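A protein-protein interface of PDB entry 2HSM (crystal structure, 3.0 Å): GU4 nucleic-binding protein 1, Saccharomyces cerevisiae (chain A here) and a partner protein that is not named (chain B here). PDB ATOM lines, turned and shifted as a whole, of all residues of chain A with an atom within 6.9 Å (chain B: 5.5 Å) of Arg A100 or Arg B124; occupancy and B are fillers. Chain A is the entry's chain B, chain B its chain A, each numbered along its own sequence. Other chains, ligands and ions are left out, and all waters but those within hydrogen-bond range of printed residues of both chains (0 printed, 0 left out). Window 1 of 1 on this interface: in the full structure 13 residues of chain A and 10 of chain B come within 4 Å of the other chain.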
ATOM      1  N   ASN A  48     -20.501  14.316   1.761  1.00  0.00           N
ATOM      2  CA  ASN A  48     -19.845  13.132   1.205  1.00  0.00           C
ATOM      3  C   ASN A  48     -20.843  11.986   0.949  1.00  0.00           C
ATOM      4  O   ASN A  48     -20.723  11.256  -0.039  1.00  0.00           O
ATOM      5  CB  ASN A  48     -18.722  12.685   2.143  1.00  0.00           C
ATOM      6  CG  ASN A  48     -17.792  11.685   1.507  1.00  0.00           C
ATOM      7  OD1 ASN A  48     -17.534  10.623   2.070  1.00  0.00           O
ATOM      8  ND2 ASN A  48     -17.265  12.018   0.341  1.00  0.00           N
ATOM      9  N   VAL A  50     -24.216  12.387   0.498  1.00  0.00           N
ATOM     10  CA  VAL A  50     -24.933  12.929  -0.664  1.00  0.00           C
ATOM     11  C   VAL A  50     -24.160  12.673  -1.966  1.00  0.00           C
ATOM     12  O   VAL A  50     -24.705  12.150  -2.944  1.00  0.00           O
ATOM     13  CB  VAL A  50     -25.151  14.451  -0.520  1.00  0.00           C
ATOM     14  CG1 VAL A  50     -25.772  15.027  -1.775  1.00  0.00           C
ATOM     15  CG2 VAL A  50     -26.003  14.771   0.709  1.00  0.00           C
ATOM     16  N   LEU A  51     -22.879  13.021  -1.968  1.00  0.00           N
ATOM     17  CA  LEU A  51     -22.063  12.842  -3.157  1.00  0.00           C
ATOM     18  C   LEU A  51     -21.708  11.385  -3.464  1.00  0.00           C
ATOM     19  O   LEU A  51     -21.137  11.114  -4.517  1.00  0.00           O
ATOM     20  CB  LEU A  51     -20.780  13.688  -3.064  1.00  0.00           C
ATOM     21  CG  LEU A  51     -20.897  15.164  -3.471  1.00  0.00           C
ATOM     22  CD1 LEU A  51     -19.516  15.808  -3.551  1.00  0.00           C
ATOM     23  CD2 LEU A  51     -21.641  15.303  -4.805  1.00  0.00           C
ATOM     24  N   ARG A  52     -22.026  10.454  -2.560  1.00  0.00           N
ATOM     25  CA  ARG A  52     -21.719   9.013  -2.782  1.00  0.00           C
ATOM     26  C   ARG A  52     -22.631   8.423  -3.857  1.00  0.00           C
ATOM     27  O   ARG A  52     -22.157   7.779  -4.799  1.00  0.00           O
ATOM     28  CB  ARG A  52     -21.825   8.193  -1.471  1.00  0.00           C
ATOM     29  CG  ARG A  52     -22.261   6.722  -1.634  1.00  0.00           C
ATOM     30  CD  ARG A  52     -21.947   5.918  -0.398  1.00  0.00           C
ATOM     31  NE  ARG A  52     -23.018   5.022   0.053  1.00  0.00           N
ATOM     32  CZ  ARG A  52     -24.191   5.414   0.561  1.00  0.00           C
ATOM     33  NH1 ARG A  52     -24.514   6.692   0.631  1.00  0.00           N
ATOM     34  NH2 ARG A  52     -25.075   4.521   0.987  1.00  0.00           N
ATOM     35  N   ASP A  53     -23.931   8.663  -3.686  1.00  0.00           N
ATOM     36  CA  ASP A  53     -24.953   8.200  -4.607  1.00  0.00           C
ATOM     37  C   ASP A  53     -25.159   9.170  -5.797  1.00  0.00           C
ATOM     38  O   ASP A  53     -25.272   8.714  -6.939  1.00  0.00           O
ATOM     39  CB  ASP A  53     -26.272   7.971  -3.854  1.00  0.00           C
ATOM     40  CG  ASP A  53     -26.124   6.996  -2.675  1.00  0.00           C
ATOM     41  OD1 ASP A  53     -25.313   6.047  -2.774  1.00  0.00           O
ATOM     42  OD2 ASP A  53     -26.830   7.177  -1.650  1.00  0.00           O
ATOM     43  N   ASN A  54     -25.183  10.486  -5.542  1.00  0.00           N
ATOM     44  CA  ASN A  54     -25.376  11.499  -6.607  1.00  0.00           C
ATOM     45  C   ASN A  54     -24.086  12.134  -7.113  1.00  0.00           C
ATOM     46  O   ASN A  54     -23.286  12.620  -6.317  1.00  0.00           O
ATOM     47  CB  ASN A  54     -26.264  12.633  -6.127  1.00  0.00           C
ATOM     48  CG  ASN A  54     -27.389  12.159  -5.267  1.00  0.00           C
ATOM     49  OD1 ASN A  54     -27.404  11.016  -4.820  1.00  0.00           O
ATOM     50  ND2 ASN A  54     -28.337  13.044  -5.004  1.00  0.00           N
ATOM     51  N   THR A  55     -23.925  12.159  -8.439  1.00  0.00           N
ATOM     52  CA  THR A  55     -22.802  12.829  -9.120  1.00  0.00           C
ATOM     53  C   THR A  55     -22.687  14.337  -8.804  1.00  0.00           C
ATOM     54  O   THR A  55     -21.580  14.867  -8.738  1.00  0.00           O
ATOM     55  CB  THR A  55     -22.884  12.626 -10.659  1.00  0.00           C
ATOM     56  OG1 THR A  55     -22.286  11.367 -11.016  1.00  0.00           O
ATOM     57  CG2 THR A  55     -22.173  13.743 -11.402  1.00  0.00           C
ATOM     58  N   PHE A  56     -23.824  15.009  -8.617  1.00  0.00           N
ATOM     59  CA  PHE A  56     -23.859  16.432  -8.257  1.00  0.00           C
ATOM     60  C   PHE A  56     -24.825  16.626  -7.113  1.00  0.00           C
ATOM     61  O   PHE A  56     -25.714  15.806  -6.889  1.00  0.00           O
ATOM     62  CB  PHE A  56     -24.270  17.308  -9.456  1.00  0.00           C
ATOM     63  CG  PHE A  56     -23.278  17.272 -10.582  1.00  0.00           C
ATOM     64  CD1 PHE A  56     -23.610  16.728 -11.803  1.00  0.00           C
ATOM     65  CD2 PHE A  56     -21.987  17.732 -10.398  1.00  0.00           C
ATOM     66  CE1 PHE A  56     -22.687  16.658 -12.819  1.00  0.00           C
ATOM     67  CE2 PHE A  56     -21.067  17.664 -11.416  1.00  0.00           C
ATOM     68  CZ  PHE A  56     -21.425  17.126 -12.630  1.00  0.00           C
ATOM     69  N   TYR A  95     -13.038  10.567   2.257  1.00  0.00           N
ATOM     70  CA  TYR A  95     -13.698  11.640   1.527  1.00  0.00           C
ATOM     71  C   TYR A  95     -13.461  11.531   0.023  1.00  0.00           C
ATOM     72  O   TYR A  95     -13.187  12.533  -0.640  1.00  0.00           O
ATOM     73  CB  TYR A  95     -13.154  12.990   1.988  1.00  0.00           C
ATOM     74  CG  TYR A  95     -13.289  13.294   3.451  1.00  0.00           C
ATOM     75  CD1 TYR A  95     -12.224  13.109   4.317  1.00  0.00           C
ATOM     76  CD2 TYR A  95     -14.470  13.821   3.960  1.00  0.00           C
ATOM     77  CE1 TYR A  95     -12.341  13.416   5.659  1.00  0.00           C
ATOM     78  CE2 TYR A  95     -14.601  14.134   5.297  1.00  0.00           C
ATOM     79  CZ  TYR A  95     -13.535  13.929   6.144  1.00  0.00           C
ATOM     80  OH  TYR A  95     -13.663  14.238   7.478  1.00  0.00           O
ATOM     81  N   ARG A  96     -13.556  10.326  -0.525  1.00  0.00           N
ATOM     82  CA  ARG A  96     -13.306  10.146  -1.959  1.00  0.00           C
ATOM     83  C   ARG A  96     -14.403  10.739  -2.860  1.00  0.00           C
ATOM     84  O   ARG A  96     -14.147  11.033  -4.024  1.00  0.00           O
ATOM     85  CB  ARG A  96     -13.088   8.671  -2.297  1.00  0.00           C
ATOM     86  CG  ARG A  96     -14.274   7.787  -2.016  1.00  0.00           C
ATOM     87  CD  ARG A  96     -14.331   6.679  -3.023  1.00  0.00           C
ATOM     88  NE  ARG A  96     -13.235   5.741  -2.823  1.00  0.00           N
ATOM     89  CZ  ARG A  96     -13.295   4.653  -2.053  1.00  0.00           C
ATOM     90  NH1 ARG A  96     -14.412   4.342  -1.383  1.00  0.00           N
ATOM     91  NH2 ARG A  96     -12.224   3.864  -1.953  1.00  0.00           N
ATOM     92  N   HIS A  97     -15.609  10.922  -2.329  1.00  0.00           N
ATOM     93  CA  HIS A  97     -16.723  11.404  -3.148  1.00  0.00           C
ATOM     94  C   HIS A  97     -16.685  12.915  -3.309  1.00  0.00           C
ATOM     95  O   HIS A  97     -16.948  13.417  -4.399  1.00  0.00           O
ATOM     96  CB  HIS A  97     -18.074  10.967  -2.582  1.00  0.00           C
ATOM     97  CG  HIS A  97     -18.119   9.529  -2.183  1.00  0.00           C
ATOM     98  ND1 HIS A  97     -17.608   8.524  -2.975  1.00  0.00           N
ATOM     99  CD2 HIS A  97     -18.601   8.928  -1.072  1.00  0.00           C
ATOM    100  CE1 HIS A  97     -17.774   7.365  -2.367  1.00  0.00           C
ATOM    101  NE2 HIS A  97     -18.382   7.582  -1.214  1.00  0.00           N
ATOM    102  N   ILE A  98     -16.359  13.636  -2.232  1.00  0.00           N
ATOM    103  CA  ILE A  98     -16.136  15.082  -2.306  1.00  0.00           C
ATOM    104  C   ILE A  98     -14.942  15.335  -3.205  1.00  0.00           C
ATOM    105  O   ILE A  98     -14.915  16.306  -3.943  1.00  0.00           O
ATOM    106  CB  ILE A  98     -15.855  15.708  -0.933  1.00  0.00           C
ATOM    107  CG1 ILE A  98     -17.075  15.575  -0.012  1.00  0.00           C
ATOM    108  CG2 ILE A  98     -15.508  17.181  -1.093  1.00  0.00           C
ATOM    109  CD1 ILE A  98     -16.797  15.848   1.448  1.00  0.00           C
ATOM    110  N   LEU A  99     -13.973  14.429  -3.161  1.00  0.00           N
ATOM    111  CA  LEU A  99     -12.759  14.554  -3.950  1.00  0.00           C
ATOM    112  C   LEU A  99     -12.963  14.430  -5.458  1.00  0.00           C
ATOM    113  O   LEU A  99     -12.318  15.158  -6.208  1.00  0.00           O
ATOM    114  CB  LEU A  99     -11.688  13.558  -3.470  1.00  0.00           C
ATOM    115  CG  LEU A  99     -10.887  14.021  -2.243  1.00  0.00           C
ATOM    116  CD1 LEU A  99     -10.255  12.859  -1.470  1.00  0.00           C
ATOM    117  CD2 LEU A  99      -9.828  15.023  -2.677  1.00  0.00           C
ATOM    118  N   ARG A 100     -13.824  13.527  -5.924  1.00  0.00           N
ATOM    119  CA  ARG A 100     -14.022  13.409  -7.380  1.00  0.00           C
ATOM    120  C   ARG A 100     -14.908  14.542  -7.891  1.00  0.00           C
ATOM    121  O   ARG A 100     -14.833  14.916  -9.061  1.00  0.00           O
ATOM    122  CB  ARG A 100     -14.569  12.038  -7.804  1.00  0.00           C
ATOM    123  CG  ARG A 100     -15.972  11.737  -7.333  1.00  0.00           C
ATOM    124  CD  ARG A 100     -16.951  11.392  -8.464  1.00  0.00           C
ATOM    125  NE  ARG A 100     -18.223  12.045  -8.185  1.00  0.00           N
ATOM    126  CZ  ARG A 100     -19.078  11.672  -7.234  1.00  0.00           C
ATOM    127  NH1 ARG A 100     -18.837  10.599  -6.480  1.00  0.00           N
ATOM    128  NH2 ARG A 100     -20.194  12.368  -7.048  1.00  0.00           N
ATOM    129  N   TRP A 101     -15.730  15.081  -6.994  1.00  0.00           N
ATOM    130  CA  TRP A 101     -16.582  16.237  -7.273  1.00  0.00           C
ATOM    131  C   TRP A 101     -15.781  17.518  -7.468  1.00  0.00           C
ATOM    132  O   TRP A 101     -16.008  18.257  -8.435  1.00  0.00           O
ATOM    133  CB  TRP A 101     -17.525  16.438  -6.104  1.00  0.00           C
ATOM    134  CG  TRP A 101     -18.443  17.583  -6.235  1.00  0.00           C
ATOM    135  CD1 TRP A 101     -19.384  17.759  -7.193  1.00  0.00           C
ATOM    136  CD2 TRP A 101     -18.556  18.700  -5.340  1.00  0.00           C
ATOM    137  NE1 TRP A 101     -20.072  18.923  -6.967  1.00  0.00           N
ATOM    138  CE2 TRP A 101     -19.586  19.523  -5.836  1.00  0.00           C
ATOM    139  CE3 TRP A 101     -17.882  19.088  -4.174  1.00  0.00           C
ATOM    140  CZ2 TRP A 101     -19.970  20.713  -5.203  1.00  0.00           C
ATOM    141  CZ3 TRP A 101     -18.261  20.270  -3.546  1.00  0.00           C
ATOM    142  CH2 TRP A 101     -19.294  21.069  -4.067  1.00  0.00           C
ATOM    143  N   ILE A 102     -14.881  17.784  -6.513  1.00  0.00           N
ATOM    144  CA  ILE A 102     -13.879  18.844  -6.627  1.00  0.00           C
ATOM    145  C   ILE A 102     -13.177  18.719  -7.967  1.00  0.00           C
ATOM    146  O   ILE A 102     -13.206  19.633  -8.784  1.00  0.00           O
ATOM    147  CB  ILE A 102     -12.789  18.739  -5.509  1.00  0.00           C
ATOM    148  CG1 ILE A 102     -13.348  19.131  -4.134  1.00  0.00           C
ATOM    149  CG2 ILE A 102     -11.582  19.613  -5.840  1.00  0.00           C
ATOM    150  CD1 ILE A 102     -13.563  20.630  -3.937  1.00  0.00           C
ATOM    151  N   ASP A 103     -12.565  17.562  -8.186  1.00  0.00           N
ATOM    152  CA  ASP A 103     -11.697  17.338  -9.333  1.00  0.00           C
ATOM    153  C   ASP A 103     -12.438  17.665 -10.605  1.00  0.00           C
ATOM    154  O   ASP A 103     -11.861  18.220 -11.538  1.00  0.00           O
ATOM    155  CB  ASP A 103     -11.228  15.881  -9.361  1.00  0.00           C
ATOM    156  CG  ASP A 103     -10.249  15.597 -10.487  1.00  0.00           C
ATOM    157  OD1 ASP A 103      -9.195  16.268 -10.556  1.00  0.00           O
ATOM    158  OD2 ASP A 103     -10.532  14.678 -11.289  1.00  0.00           O
ATOM    159  N   TYR A 104     -13.723  17.329 -10.631  1.00  0.00           N
ATOM    160  CA  TYR A 104     -14.543  17.667 -11.771  1.00  0.00           C
ATOM    161  C   TYR A 104     -14.648  19.182 -11.870  1.00  0.00           C
ATOM    162  O   TYR A 104     -14.136  19.784 -12.801  1.00  0.00           O
ATOM    163  CB  TYR A 104     -15.931  17.026 -11.678  1.00  0.00           C
ATOM    164  CG  TYR A 104     -16.726  17.225 -12.937  1.00  0.00           C
ATOM    165  CD1 TYR A 104     -16.396  16.534 -14.087  1.00  0.00           C
ATOM    166  CD2 TYR A 104     -17.777  18.134 -12.997  1.00  0.00           C
ATOM    167  CE1 TYR A 104     -17.101  16.719 -15.266  1.00  0.00           C
ATOM    168  CE2 TYR A 104     -18.493  18.329 -14.176  1.00  0.00           C
ATOM    169  CZ  TYR A 104     -18.144  17.611 -15.306  1.00  0.00           C
ATOM    170  OH  TYR A 104     -18.816  17.766 -16.492  1.00  0.00           O
ATOM    171  N   MET A 105     -15.263  19.798 -10.878  1.00  0.00           N
ATOM    172  CA  MET A 105     -15.605  21.207 -10.973  1.00  0.00           C
ATOM    173  C   MET A 105     -14.444  22.183 -11.017  1.00  0.00           C
ATOM    174  O   MET A 105     -14.584  23.270 -11.582  1.00  0.00           O
ATOM    175  CB  MET A 105     -16.505  21.596  -9.825  1.00  0.00           C
ATOM    176  CG  MET A 105     -17.832  20.941  -9.922  1.00  0.00           C
ATOM    177  SD  MET A 105     -19.119  22.137  -9.637  1.00  0.00           S
ATOM    178  CE  MET A 105     -20.500  21.019  -9.560  1.00  0.00           C
ATOM    179  N   ILE A 119      -4.686  15.755  -6.169  1.00  0.00           N
ATOM    180  CA  ILE A 119      -5.435  14.688  -6.845  1.00  0.00           C
ATOM    181  C   ILE A 119      -4.504  13.615  -7.447  1.00  0.00           C
ATOM    182  O   ILE A 119      -3.906  13.814  -8.509  1.00  0.00           O
ATOM    183  CB  ILE A 119      -6.432  15.278  -7.901  1.00  0.00           C
ATOM    184  CG1 ILE A 119      -7.853  14.801  -7.602  1.00  0.00           C
ATOM    185  CG2 ILE A 119      -6.007  14.965  -9.344  1.00  0.00           C
ATOM    186  CD1 ILE A 119      -8.445  15.437  -6.363  1.00  0.00           C
ATOM    187  N   HIS A 121      -4.870   9.715  -7.869  1.00  0.00           N
ATOM    188  CA  HIS A 121      -5.288   8.601  -8.689  1.00  0.00           C
ATOM    189  C   HIS A 121      -4.406   7.382  -8.486  1.00  0.00           C
ATOM    190  O   HIS A 121      -3.277   7.337  -8.966  1.00  0.00           O
ATOM    191  CB  HIS A 121      -5.303   9.022 -10.149  1.00  0.00           C
ATOM    192  CG  HIS A 121      -6.366  10.019 -10.471  1.00  0.00           C
ATOM    193  ND1 HIS A 121      -7.700   9.684 -10.533  1.00  0.00           N
ATOM    194  CD2 HIS A 121      -6.297  11.343 -10.732  1.00  0.00           C
ATOM    195  CE1 HIS A 121      -8.406  10.759 -10.824  1.00  0.00           C
ATOM    196  NE2 HIS A 121      -7.579  11.780 -10.950  1.00  0.00           N
ATOM    197  N   GLN B 120     -12.240   1.845 -10.851  1.00  0.00           N
ATOM    198  CA  GLN B 120     -11.909   2.806 -11.893  1.00  0.00           C
ATOM    199  C   GLN B 120     -12.647   4.120 -11.672  1.00  0.00           C
ATOM    200  O   GLN B 120     -12.123   5.163 -12.003  1.00  0.00           O
ATOM    201  CB  GLN B 120     -12.257   2.213 -13.263  1.00  0.00           C
ATOM    202  CG  GLN B 120     -12.021   3.105 -14.456  1.00  0.00           C
ATOM    203  CD  GLN B 120     -10.577   3.534 -14.626  1.00  0.00           C
ATOM    204  OE1 GLN B 120     -10.305   4.688 -14.976  1.00  0.00           O
ATOM    205  NE2 GLN B 120      -9.644   2.614 -14.395  1.00  0.00           N
ATOM    206  N   LEU B 121     -13.840   4.071 -11.083  1.00  0.00           N
ATOM    207  CA  LEU B 121     -14.716   5.239 -10.972  1.00  0.00           C
ATOM    208  C   LEU B 121     -14.608   5.961  -9.634  1.00  0.00           C
ATOM    209  O   LEU B 121     -15.466   6.788  -9.289  1.00  0.00           O
ATOM    210  CB  LEU B 121     -16.174   4.798 -11.186  1.00  0.00           C
ATOM    211  CG  LEU B 121     -16.676   4.712 -12.626  1.00  0.00           C
ATOM    212  CD1 LEU B 121     -17.891   3.789 -12.703  1.00  0.00           C
ATOM    213  CD2 LEU B 121     -17.002   6.109 -13.170  1.00  0.00           C
ATOM    214  N   ASN B 122     -13.566   5.654  -8.874  1.00  0.00           N
ATOM    215  CA  ASN B 122     -13.473   6.139  -7.492  1.00  0.00           C
ATOM    216  C   ASN B 122     -13.326   7.642  -7.392  1.00  0.00           C
ATOM    217  O   ASN B 122     -14.065   8.298  -6.659  1.00  0.00           O
ATOM    218  CB  ASN B 122     -12.297   5.479  -6.768  1.00  0.00           C
ATOM    219  CG  ASN B 122     -12.702   4.251  -6.009  1.00  0.00           C
ATOM    220  OD1 ASN B 122     -12.104   3.193  -6.161  1.00  0.00           O
ATOM    221  ND2 ASN B 122     -13.729   4.384  -5.179  1.00  0.00           N
ATOM    222  N   LEU B 123     -12.349   8.159  -8.132  1.00  0.00           N
ATOM    223  CA  LEU B 123     -12.061   9.585  -8.182  1.00  0.00           C
ATOM    224  C   LEU B 123     -12.446  10.176  -9.548  1.00  0.00           C
ATOM    225  O   LEU B 123     -11.743  11.046 -10.075  1.00  0.00           O
ATOM    226  CB  LEU B 123     -10.569   9.811  -7.915  1.00  0.00           C
ATOM    227  CG  LEU B 123     -10.041   9.363  -6.553  1.00  0.00           C
ATOM    228  CD1 LEU B 123      -8.532   9.519  -6.509  1.00  0.00           C
ATOM    229  CD2 LEU B 123     -10.716  10.142  -5.404  1.00  0.00           C
ATOM    230  N   ARG B 124     -13.557   9.704 -10.115  1.00  0.00           N
ATOM    231  CA  ARG B 124     -13.948  10.062 -11.488  1.00  0.00           C
ATOM    232  C   ARG B 124     -15.455  10.267 -11.648  1.00  0.00           C
ATOM    233  O   ARG B 124     -16.265   9.783 -10.847  1.00  0.00           O
ATOM    234  CB  ARG B 124     -13.488   8.988 -12.471  1.00  0.00           C
ATOM    235  CG  ARG B 124     -12.022   9.056 -12.838  1.00  0.00           C
ATOM    236  CD  ARG B 124     -11.555   7.712 -13.316  1.00  0.00           C
ATOM    237  NE  ARG B 124     -10.482   7.778 -14.301  1.00  0.00           N
ATOM    238  CZ  ARG B 124      -9.219   7.397 -14.103  1.00  0.00           C
ATOM    239  NH1 ARG B 124      -8.808   6.901 -12.936  1.00  0.00           N
ATOM    240  NH2 ARG B 124      -8.345   7.509 -15.094  1.00  0.00           N
ATOM    241  N   THR B 125     -15.815  11.005 -12.690  1.00  0.00           N
ATOM    242  CA  THR B 125     -17.206  11.206 -13.059  1.00  0.00           C
ATOM    243  C   THR B 125     -17.498  10.377 -14.300  1.00  0.00           C
ATOM    244  O   THR B 125     -18.594   9.835 -14.440  1.00  0.00           O
ATOM    245  CB  THR B 125     -17.496  12.703 -13.256  1.00  0.00           C
ATOM    246  OG1 THR B 125     -17.130  13.401 -12.056  1.00  0.00           O
ATOM    247  CG2 THR B 125     -18.967  12.956 -13.546  1.00  0.00           C
ATOM    248  N   PHE B 126     -16.496  10.257 -15.173  1.00  0.00           N
ATOM    249  CA  PHE B 126     -16.547   9.391 -16.347  1.00  0.00           C
ATOM    250  C   PHE B 126     -15.390   8.421 -16.337  1.00  0.00           C
ATOM    251  O   PHE B 126     -14.368   8.652 -15.684  1.00  0.00           O
ATOM    252  CB  PHE B 126     -16.553  10.221 -17.639  1.00  0.00           C
ATOM    253  CG  PHE B 126     -17.698  11.169 -17.697  1.00  0.00           C
ATOM    254  CD1 PHE B 126     -17.506  12.526 -17.501  1.00  0.00           C
ATOM    255  CD2 PHE B 126     -18.990  10.689 -17.843  1.00  0.00           C
ATOM    256  CE1 PHE B 126     -18.570  13.389 -17.492  1.00  0.00           C
ATOM    257  CE2 PHE B 126     -20.071  11.558 -17.833  1.00  0.00           C
ATOM    258  CZ  PHE B 126     -19.859  12.908 -17.659  1.00  0.00           C
ATOM    259  N   ILE B 127     -15.562   7.344 -17.094  1.00  0.00           N
ATOM    260  CA  ILE B 127     -14.678   6.185 -17.034  1.00  0.00           C
ATOM    261  C   ILE B 127     -13.222   6.565 -17.254  1.00  0.00           C
ATOM    262  O   ILE B 127     -12.401   6.325 -16.382  1.00  0.00           O
ATOM    263  CB  ILE B 127     -15.104   5.114 -18.050  1.00  0.00           C
ATOM    264  CG1 ILE B 127     -16.497   4.571 -17.694  1.00  0.00           C
ATOM    265  CG2 ILE B 127     -14.090   3.993 -18.088  1.00  0.00           C
ATOM    266  CD1 ILE B 127     -16.939   3.414 -18.552  1.00  0.00           C
ATOM    267  N   LEU B 128     -12.924   7.171 -18.405  1.00  0.00           N
ATOM    268  CA  LEU B 128     -11.551   7.565 -18.785  1.00  0.00           C
ATOM    269  C   LEU B 128     -11.127   8.901 -18.158  1.00  0.00           C
ATOM    270  O   LEU B 128      -9.997   9.354 -18.357  1.00  0.00           O
ATOM    271  CB  LEU B 128     -11.400   7.644 -20.312  1.00  0.00           C
ATOM    272  CG  LEU B 128     -11.165   6.348 -21.091  1.00  0.00           C
ATOM    273  CD1 LEU B 128     -11.406   6.571 -22.592  1.00  0.00           C
ATOM    274  CD2 LEU B 128      -9.762   5.793 -20.855  1.00  0.00           C
ATOM    275  N   GLY B 129     -12.033   9.536 -17.420  1.00  0.00           N
ATOM    276  CA  GLY B 129     -11.667  10.660 -16.566  1.00  0.00           C
ATOM    277  C   GLY B 129     -11.972  12.067 -17.063  1.00  0.00           C
ATOM    278  O   GLY B 129     -11.829  13.024 -16.301  1.00  0.00           O
ATOM    279  N   ARG B 164     -23.931   5.251  -9.089  1.00  0.00           N
ATOM    280  CA  ARG B 164     -23.952   6.710  -9.238  1.00  0.00           C
ATOM    281  C   ARG B 164     -23.715   7.111 -10.690  1.00  0.00           C
ATOM    282  O   ARG B 164     -24.474   7.894 -11.259  1.00  0.00           O
ATOM    283  CB  ARG B 164     -22.870   7.324  -8.354  1.00  0.00           C
ATOM    284  CG  ARG B 164     -22.654   8.804  -8.524  1.00  0.00           C
ATOM    285  CD  ARG B 164     -21.200   9.128  -8.298  1.00  0.00           C
ATOM    286  NE  ARG B 164     -20.352   8.771  -9.432  1.00  0.00           N
ATOM    287  CZ  ARG B 164     -19.148   8.217  -9.328  1.00  0.00           C
ATOM    288  NH1 ARG B 164     -18.648   7.899  -8.136  1.00  0.00           N
ATOM    289  NH2 ARG B 164     -18.435   7.944 -10.423  1.00  0.00           N
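The side-chain amide nitrogen (ND2) of Asn B122 sits close to the guanidinium group (NE) of Arg A96 (2.8 Å).
The guanidinium group (NH1) of Arg A100 lies close to the guanidinium group (NH1) of Arg B164, at 3.2 Å.
The guanidinium group (NH2) of Arg B164 sits at hydrogen-bond distance from the backbone carbonyl oxygen (O) of Arg B124 (2.9 Å).
The guanidinium group of Arg A52 lies within salt-bridge range of the side-chain carboxylate of Asp A53, 3.3 Å away.
NE of Arg B124 sits at hydrogen-bond distance from O of Ile B127 (3.2 Å).
OD1 of Asn A54 lies close to O of Val A50 (3.5 Å).
The guanidinium group of Arg A100 is in hydrogen-bond range of the backbone carbonyl oxygen of Leu A51 (3.0 Å).
O of Thr A55 is in hydrogen-bond range of NH2 of Arg A100.
Arg B164 touches Arg A52.
O of Asp A53 touches CG of Arg B164 (3.1 Å).
Thr B125 touches Thr A55.
N of Thr A55 touches CG of Arg B164, 3.6 Å away.
Leu B123 touches Arg A96 (CD2 to O, 3.8 Å).
Arg A100 touches Leu B123.
CD of Arg A100 touches O of Arg B124 (3.0 Å).
CD1 of Tyr A104 touches OG1 of Thr B125, at 3.8 Å.
O of Leu B123 touches CE1 of His A121, 3.4 Å away.
NH1 of Arg B124 touches ND1 of His A121, 3.8 Å away.
Of chain B, only Asn B122, Leu B123, Arg B124 and Arg B164 come within 4 Å of Arg A100.
Of the printed residues of chain A, Arg B124 touches Arg A100 and His A121.
Printed residues of chain B within 4 Å of Thr A55: Thr B125 and Arg B164.
Of the printed residues of chain A, Asn B122 touches Arg A96 and Arg A100.
Printed residues of chain A within 4 Å of Thr B125: Thr A55 (3.9 Å) and Tyr A104 (3.8 Å).
Ile A119 touches none of the printed residues of chain B.
The nearest residue of chain B that does not touch Arg A100 is Thr B125 (4.1 Å).
Hydrophobic or aromatic side chains of chain A that line the printed part of chain B: Tyr A104 and His A121.
Of the 11 printed residues of chain B, 5 touch a printed residue of chain A.
Printed residues of chain B that touch a printed residue of chain A: Asn B122, Leu B123, Arg B124, Thr B125 and Arg B164.
Hydrophobic or aromatic side chains of chain B within 4 Å of the printed part of chain A: Leu B123.
Among the printed residues, no Asp or Glu carboxylate lies within 4 Å of a Lys or Arg side-chain nitrogen of the other chain.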
